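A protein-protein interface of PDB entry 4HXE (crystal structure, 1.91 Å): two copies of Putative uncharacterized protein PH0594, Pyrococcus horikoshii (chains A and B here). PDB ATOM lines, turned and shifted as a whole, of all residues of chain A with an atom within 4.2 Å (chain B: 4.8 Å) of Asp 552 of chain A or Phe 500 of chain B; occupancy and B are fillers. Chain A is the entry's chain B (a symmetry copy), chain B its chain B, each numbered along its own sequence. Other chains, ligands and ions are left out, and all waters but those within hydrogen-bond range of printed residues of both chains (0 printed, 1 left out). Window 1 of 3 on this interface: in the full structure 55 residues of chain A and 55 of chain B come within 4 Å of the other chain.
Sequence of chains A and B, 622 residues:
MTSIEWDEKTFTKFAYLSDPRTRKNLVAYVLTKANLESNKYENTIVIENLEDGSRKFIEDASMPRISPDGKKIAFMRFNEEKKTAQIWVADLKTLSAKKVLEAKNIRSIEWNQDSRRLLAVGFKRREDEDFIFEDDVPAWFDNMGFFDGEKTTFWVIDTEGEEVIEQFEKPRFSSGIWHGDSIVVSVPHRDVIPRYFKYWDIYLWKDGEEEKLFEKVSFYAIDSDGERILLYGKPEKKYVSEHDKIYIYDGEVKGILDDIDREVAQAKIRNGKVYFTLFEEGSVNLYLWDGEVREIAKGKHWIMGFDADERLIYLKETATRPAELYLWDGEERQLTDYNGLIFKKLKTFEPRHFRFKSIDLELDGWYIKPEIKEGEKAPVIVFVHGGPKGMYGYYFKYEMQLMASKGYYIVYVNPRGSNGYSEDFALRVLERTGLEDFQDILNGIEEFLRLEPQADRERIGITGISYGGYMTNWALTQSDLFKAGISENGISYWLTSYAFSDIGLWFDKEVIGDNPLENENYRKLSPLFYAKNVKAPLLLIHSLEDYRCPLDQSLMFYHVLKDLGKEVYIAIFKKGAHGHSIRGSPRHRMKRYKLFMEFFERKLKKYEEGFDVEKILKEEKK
Printed residues of chain B within 4 Å of Thr 496 of chain A: Thr 496 (3.2 Å).
Asp 552 of chain A touches one residue of chain B.
Gln 553 of chain A touches none of the printed residues of chain B.
Of the printed residues of chain B, Met 556 of chain A touches Thr 496 (3.7 Å), Ala 499 (3.5 Å) and Phe 500 (3.7 Å).
Printed residues of chain A within 4 Å of Trp 140 of chain B: Leu 551 and Leu 555.
Of chain A, only Asp 552 (3.4 Å), Leu 555 (3.7 Å), Met 556 (3.7 Å) and His 559 (3.8 Å) come within 4 Å of Phe 500 of chain B.
Printed residues of chain A within 4 Å of Asp 552 of chain B: Phe 500 (3.4 Å).
The nearest printed residue of chain B that does not touch Asp 552 of chain A is Thr 496 of chain B (5.2 Å).
The nearest printed residue of chain A that does not touch Ala 499 of chain B is Asp 552 of chain A (6.3 Å).
Printed residues of chain A that touch a printed residue of chain B: Thr 496, Phe 500, Leu 551, Asp 552, Leu 555, Met 556 and His 559.
Hydrophobic or aromatic side chains of chain A that line the printed part of chain B: Phe 500, Leu 551, Leu 555, Met 556 and His 559.
Hydrophobic or aromatic side chains of chain B that line the printed part of chain A: Trp 140, Ala 499 and Phe 500.
Among the printed residues, no Asp or Glu carboxylate lies within 4 Å of a Lys or Arg side-chain nitrogen of the other chain.
Thr 496 of chain B touches its own counterpart, Thr 496 of chain A.
Phe 500 of chain A touches Asp 552 of chain B, and with the chains exchanged Asp 552 of chain A touches Phe 500 of chain B.
4 positions are printed for both chains.
The backbone carbonyl oxygen (O) of Ala 499 of chain B is in hydrogen-bond range of a ring nitrogen (ND1) of His 559 of chain A (2.8 Å).
NE1 of Trp 140 of chain B sits at hydrogen-bond distance from O of Phe 500 of chain B (2.9 Å).
The side-chain carboxylate (OD1) of Asp 552 of chain B lies within hydrogen-bond range of the side-chain hydroxyl (OG1) of Thr 496 of chain B, 2.7 Å away.
The side-chain hydroxyl (OG1) of Thr 496 of chain A lies within hydrogen-bond range of the side-chain carboxylate (OD1) of Asp 552 of chain A.
The side-chain amide nitrogen (NE2) of Gln 553 of chain A is in hydrogen-bond range of the side-chain hydroxyl (OG1) of Thr 496 of chain A (2.8 Å).
Among the printed residues, pairs that only touch across the chains: Thr 496 of chain A with Thr 496 of chain B, Phe 500 of chain A with Asp 552 of chain B, Asp 552 of chain A with Phe 500 of chain B, Met 556 of chain A with Ala 499 of chain B, Leu 555 of chain A with Phe 500 of chain B, Met 556 of chain A with Phe 500 of chain B, Leu 555 of chain A with Trp 140 of chain B, Met 556 of chain A with Thr 496 of chain B, His 559 of chain A with Phe 500 of chain B, Leu 551 of chain A with Trp 140 of chain B and Leu 555 of chain A with Ala 499 of chain B.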
ATOM      1  N   THR A 496      19.668 -19.857 -29.281  1.00  0.00           N
ATOM      2  CA  THR A 496      20.820 -20.094 -30.163  1.00  0.00           C
ATOM      3  C   THR A 496      20.749 -21.431 -30.871  1.00  0.00           C
ATOM      4  O   THR A 496      21.396 -21.617 -31.916  1.00  0.00           O
ATOM      5  CB  THR A 496      22.164 -19.934 -29.401  1.00  0.00           C
ATOM      6  OG1 THR A 496      22.251 -20.984 -28.436  1.00  0.00           O
ATOM      7  CG2 THR A 496      22.191 -18.567 -28.729  1.00  0.00           C
ATOM      8  N   PHE A 500      21.431 -21.012 -34.660  1.00  0.00           N
ATOM      9  CA  PHE A 500      22.799 -21.454 -34.934  1.00  0.00           C
ATOM     10  C   PHE A 500      22.878 -22.903 -35.466  1.00  0.00           C
ATOM     11  O   PHE A 500      23.782 -23.225 -36.266  1.00  0.00           O
ATOM     12  CB  PHE A 500      23.645 -21.255 -33.651  1.00  0.00           C
ATOM     13  CG  PHE A 500      25.168 -21.223 -33.848  1.00  0.00           C
ATOM     14  CD1 PHE A 500      25.765 -20.685 -35.011  1.00  0.00           C
ATOM     15  CD2 PHE A 500      26.001 -21.681 -32.804  1.00  0.00           C
ATOM     16  CE1 PHE A 500      27.168 -20.626 -35.140  1.00  0.00           C
ATOM     17  CE2 PHE A 500      27.423 -21.604 -32.932  1.00  0.00           C
ATOM     18  CZ  PHE A 500      27.988 -21.093 -34.099  1.00  0.00           C
ATOM     19  N   PRO A 550      25.459 -26.873 -31.391  1.00  0.00           N
ATOM     20  CA  PRO A 550      26.775 -26.322 -31.592  1.00  0.00           C
ATOM     21  C   PRO A 550      27.409 -25.999 -30.230  1.00  0.00           C
ATOM     22  O   PRO A 550      26.735 -26.008 -29.171  1.00  0.00           O
ATOM     23  CB  PRO A 550      26.492 -25.051 -32.455  1.00  0.00           C
ATOM     24  CG  PRO A 550      25.145 -25.350 -33.122  1.00  0.00           C
ATOM     25  CD  PRO A 550      24.400 -26.033 -32.011  1.00  0.00           C
ATOM     26  N   LEU A 551      28.705 -25.732 -30.260  1.00  0.00           N
ATOM     27  CA  LEU A 551      29.553 -25.585 -29.070  1.00  0.00           C
ATOM     28  C   LEU A 551      29.016 -24.572 -28.080  1.00  0.00           C
ATOM     29  O   LEU A 551      29.199 -24.685 -26.847  1.00  0.00           O
ATOM     30  CB  LEU A 551      30.955 -25.125 -29.562  1.00  0.00           C
ATOM     31  CG  LEU A 551      32.008 -24.992 -28.432  1.00  0.00           C
ATOM     32  CD1 LEU A 551      32.265 -26.321 -27.689  1.00  0.00           C
ATOM     33  CD2 LEU A 551      33.321 -24.339 -28.978  1.00  0.00           C
ATOM     34  N   ASP A 552      28.386 -23.518 -28.575  1.00  0.00           N
ATOM     35  CA  ASP A 552      27.953 -22.501 -27.592  1.00  0.00           C
ATOM     36  C   ASP A 552      26.993 -23.085 -26.518  1.00  0.00           C
ATOM     37  O   ASP A 552      26.894 -22.578 -25.398  1.00  0.00           O
ATOM     38  CB  ASP A 552      27.203 -21.342 -28.284  1.00  0.00           C
ATOM     39  CG  ASP A 552      25.936 -21.838 -28.966  1.00  0.00           C
ATOM     40  OD1 ASP A 552      24.889 -21.219 -28.721  1.00  0.00           O
ATOM     41  OD2 ASP A 552      25.970 -22.878 -29.721  1.00  0.00           O
ATOM     42  N   GLN A 553      26.286 -24.152 -26.858  1.00  0.00           N
ATOM     43  CA  GLN A 553      25.351 -24.741 -25.925  1.00  0.00           C
ATOM     44  C   GLN A 553      26.100 -25.224 -24.655  1.00  0.00           C
ATOM     45  O   GLN A 553      25.534 -25.158 -23.561  1.00  0.00           O
ATOM     46  CB  GLN A 553      24.595 -25.901 -26.608  1.00  0.00           C
ATOM     47  CG  GLN A 553      23.743 -25.424 -27.808  1.00  0.00           C
ATOM     48  CD  GLN A 553      22.617 -24.532 -27.332  1.00  0.00           C
ATOM     49  OE1 GLN A 553      22.283 -24.530 -26.135  1.00  0.00           O
ATOM     50  NE2 GLN A 553      22.008 -23.759 -28.262  1.00  0.00           N
ATOM     51  N   SER A 554      27.310 -25.757 -24.815  1.00  0.00           N
ATOM     52  CA  SER A 554      28.081 -26.181 -23.656  1.00  0.00           C
ATOM     53  C   SER A 554      28.944 -25.063 -23.141  1.00  0.00           C
ATOM     54  O   SER A 554      28.921 -24.808 -21.958  1.00  0.00           O
ATOM     55  CB  SER A 554      28.979 -27.402 -23.967  1.00  0.00           C
ATOM     56  OG  SER A 554      28.207 -28.562 -24.077  1.00  0.00           O
ATOM     57  N   LEU A 555      29.660 -24.364 -24.036  1.00  0.00           N
ATOM     58  CA  LEU A 555      30.643 -23.400 -23.579  1.00  0.00           C
ATOM     59  C   LEU A 555      29.948 -22.187 -22.902  1.00  0.00           C
ATOM     60  O   LEU A 555      30.484 -21.631 -21.951  1.00  0.00           O
ATOM     61  CB  LEU A 555      31.569 -22.949 -24.745  1.00  0.00           C
ATOM     62  CG  LEU A 555      32.695 -21.987 -24.325  1.00  0.00           C
ATOM     63  CD1 LEU A 555      33.487 -22.526 -23.098  1.00  0.00           C
ATOM     64  CD2 LEU A 555      33.606 -21.804 -25.541  1.00  0.00           C
ATOM     65  N   MET A 556      28.766 -21.771 -23.386  1.00  0.00           N
ATOM     66  CA  MET A 556      28.046 -20.656 -22.718  1.00  0.00           C
ATOM     67  C   MET A 556      27.649 -21.072 -21.302  1.00  0.00           C
ATOM     68  O   MET A 556      27.781 -20.282 -20.365  1.00  0.00           O
ATOM     69  CB  MET A 556      26.801 -20.203 -23.496  1.00  0.00           C
ATOM     70  CG  MET A 556      27.134 -19.498 -24.829  1.00  0.00           C
ATOM     71  SD  MET A 556      25.597 -18.726 -25.484  1.00  0.00           S
ATOM     72  CE  MET A 556      24.497 -20.155 -25.638  1.00  0.00           C
ATOM     73  N   HIS A 559      30.881 -21.159 -19.132  1.00  0.00           N
ATOM     74  CA  HIS A 559      31.358 -19.842 -18.761  1.00  0.00           C
ATOM     75  C   HIS A 559      30.421 -19.185 -17.734  1.00  0.00           C
ATOM     76  O   HIS A 559      30.878 -18.559 -16.765  1.00  0.00           O
ATOM     77  CB  HIS A 559      31.391 -18.911 -19.992  1.00  0.00           C
ATOM     78  CG  HIS A 559      32.559 -19.112 -20.848  1.00  0.00           C
ATOM     79  ND1 HIS A 559      32.564 -18.763 -22.168  1.00  0.00           N
ATOM     80  CD2 HIS A 559      33.853 -19.608 -20.553  1.00  0.00           C
ATOM     81  CE1 HIS A 559      33.801 -19.041 -22.701  1.00  0.00           C
ATOM     82  NE2 HIS A 559      34.584 -19.573 -21.718  1.00  0.00           N
ATOM     83  N   TRP B 140      38.926 -19.862 -24.101  1.00  0.00           N
ATOM     84  CA  TRP B 140      39.684 -19.486 -25.311  1.00  0.00           C
ATOM     85  C   TRP B 140      39.897 -18.014 -25.380  1.00  0.00           C
ATOM     86  O   TRP B 140      39.291 -17.277 -24.605  1.00  0.00           O
ATOM     87  CB  TRP B 140      38.948 -19.997 -26.561  1.00  0.00           C
ATOM     88  CG  TRP B 140      37.505 -19.491 -26.721  1.00  0.00           C
ATOM     89  CD1 TRP B 140      36.846 -18.436 -26.024  1.00  0.00           C
ATOM     90  CD2 TRP B 140      36.548 -19.971 -27.695  1.00  0.00           C
ATOM     91  NE1 TRP B 140      35.567 -18.249 -26.490  1.00  0.00           N
ATOM     92  CE2 TRP B 140      35.326 -19.156 -27.521  1.00  0.00           C
ATOM     93  CE3 TRP B 140      36.574 -20.977 -28.683  1.00  0.00           C
ATOM     94  CZ2 TRP B 140      34.209 -19.347 -28.313  1.00  0.00           C
ATOM     95  CZ3 TRP B 140      35.431 -21.178 -29.463  1.00  0.00           C
ATOM     96  CH2 TRP B 140      34.276 -20.375 -29.287  1.00  0.00           C
ATOM     97  N   THR B 496      24.852 -13.860 -26.234  1.00  0.00           N
ATOM     98  CA  THR B 496      25.861 -14.878 -26.557  1.00  0.00           C
ATOM     99  C   THR B 496      27.267 -14.318 -26.594  1.00  0.00           C
ATOM    100  O   THR B 496      28.243 -15.075 -26.453  1.00  0.00           O
ATOM    101  CB  THR B 496      25.520 -15.621 -27.878  1.00  0.00           C
ATOM    102  OG1 THR B 496      25.625 -14.684 -28.951  1.00  0.00           O
ATOM    103  CG2 THR B 496      24.107 -16.183 -27.778  1.00  0.00           C
ATOM    104  N   SER B 497      27.375 -12.991 -26.775  1.00  0.00           N
ATOM    105  CA  SER B 497      28.646 -12.360 -26.736  1.00  0.00           C
ATOM    106  C   SER B 497      29.102 -12.507 -25.296  1.00  0.00           C
ATOM    107  O   SER B 497      30.246 -12.877 -25.024  1.00  0.00           O
ATOM    108  CB  SER B 497      28.529 -10.886 -27.112  1.00  0.00           C
ATOM    109  OG  SER B 497      29.720 -10.205 -26.737  1.00  0.00           O
ATOM    110  N   TYR B 498      28.201 -12.203 -24.357  1.00  0.00           N
ATOM    111  CA  TYR B 498      28.557 -12.292 -22.957  1.00  0.00           C
ATOM    112  C   TYR B 498      29.069 -13.703 -22.526  1.00  0.00           C
ATOM    113  O   TYR B 498      30.117 -13.841 -21.837  1.00  0.00           O
ATOM    114  CB  TYR B 498      27.349 -11.790 -22.092  1.00  0.00           C
ATOM    115  CG  TYR B 498      27.363 -12.409 -20.685  1.00  0.00           C
ATOM    116  CD1 TYR B 498      28.290 -11.989 -19.735  1.00  0.00           C
ATOM    117  CD2 TYR B 498      26.479 -13.442 -20.354  1.00  0.00           C
ATOM    118  CE1 TYR B 498      28.328 -12.549 -18.471  1.00  0.00           C
ATOM    119  CE2 TYR B 498      26.510 -14.036 -19.098  1.00  0.00           C
ATOM    120  CZ  TYR B 498      27.418 -13.571 -18.166  1.00  0.00           C
ATOM    121  OH  TYR B 498      27.433 -14.170 -16.932  1.00  0.00           O
ATOM    122  N   ALA B 499      28.340 -14.738 -22.976  1.00  0.00           N
ATOM    123  CA  ALA B 499      28.475 -16.075 -22.424  1.00  0.00           C
ATOM    124  C   ALA B 499      29.448 -16.912 -23.275  1.00  0.00           C
ATOM    125  O   ALA B 499      30.037 -17.826 -22.736  1.00  0.00           O
ATOM    126  CB  ALA B 499      27.099 -16.783 -22.348  1.00  0.00           C
ATOM    127  N   PHE B 500      29.680 -16.535 -24.529  1.00  0.00           N
ATOM    128  CA  PHE B 500      30.469 -17.347 -25.457  1.00  0.00           C
ATOM    129  C   PHE B 500      31.867 -16.756 -25.749  1.00  0.00           C
ATOM    130  O   PHE B 500      32.827 -17.518 -25.988  1.00  0.00           O
ATOM    131  CB  PHE B 500      29.641 -17.556 -26.751  1.00  0.00           C
ATOM    132  CG  PHE B 500      30.076 -18.726 -27.646  1.00  0.00           C
ATOM    133  CD1 PHE B 500      30.611 -19.922 -27.112  1.00  0.00           C
ATOM    134  CD2 PHE B 500      29.871 -18.633 -29.039  1.00  0.00           C
ATOM    135  CE1 PHE B 500      30.956 -20.996 -27.958  1.00  0.00           C
ATOM    136  CE2 PHE B 500      30.206 -19.732 -29.891  1.00  0.00           C
ATOM    137  CZ  PHE B 500      30.757 -20.890 -29.345  1.00  0.00           C
ATOM    138  N   SER B 501      32.014 -15.425 -25.753  1.00  0.00           N
ATOM    139  CA  SER B 501      33.281 -14.849 -26.353  1.00  0.00           C
ATOM    140  C   SER B 501      34.399 -14.922 -25.329  1.00  0.00           C
ATOM    141  O   SER B 501      34.142 -15.325 -24.156  1.00  0.00           O
ATOM    142  CB  SER B 501      33.061 -13.402 -26.766  1.00  0.00           C
ATOM    143  OG  SER B 501      32.892 -12.640 -25.570  1.00  0.00           O
ATOM    144  N   ASP B 502      35.630 -14.591 -25.728  1.00  0.00           N
ATOM    145  CA  ASP B 502      36.765 -14.682 -24.805  1.00  0.00           C
ATOM    146  C   ASP B 502      36.626 -13.682 -23.656  1.00  0.00           C
ATOM    147  O   ASP B 502      37.006 -13.981 -22.516  1.00  0.00           O
ATOM    148  CB  ASP B 502      38.100 -14.492 -25.510  1.00  0.00           C
ATOM    149  CG  ASP B 502      38.141 -13.269 -26.420  1.00  0.00           C
ATOM    150  OD1 ASP B 502      37.147 -12.474 -26.514  1.00  0.00           O
ATOM    151  OD2 ASP B 502      39.188 -13.142 -27.082  1.00  0.00           O
ATOM    152  N   PRO B 550      32.461 -14.632 -31.594  1.00  0.00           N
ATOM    153  CA  PRO B 550      32.489 -15.963 -32.141  1.00  0.00           C
ATOM    154  C   PRO B 550      31.475 -16.066 -33.292  1.00  0.00           C
ATOM    155  O   PRO B 550      30.622 -15.169 -33.500  1.00  0.00           O
ATOM    156  CB  PRO B 550      32.115 -16.853 -30.913  1.00  0.00           C
ATOM    157  CG  PRO B 550      32.491 -15.989 -29.705  1.00  0.00           C
ATOM    158  CD  PRO B 550      32.062 -14.624 -30.161  1.00  0.00           C
ATOM    159  N   ASP B 552      28.815 -17.569 -34.009  1.00  0.00           N
ATOM    160  CA  ASP B 552      27.341 -17.477 -33.929  1.00  0.00           C
ATOM    161  C   ASP B 552      26.822 -16.033 -34.178  1.00  0.00           C
ATOM    162  O   ASP B 552      25.685 -15.823 -34.610  1.00  0.00           O
ATOM    163  CB  ASP B 552      26.831 -17.904 -32.535  1.00  0.00           C
ATOM    164  CG  ASP B 552      27.372 -16.986 -31.449  1.00  0.00           C
ATOM    165  OD1 ASP B 552      26.547 -16.517 -30.650  1.00  0.00           O
ATOM    166  OD2 ASP B 552      28.623 -16.693 -31.410  1.00  0.00           O
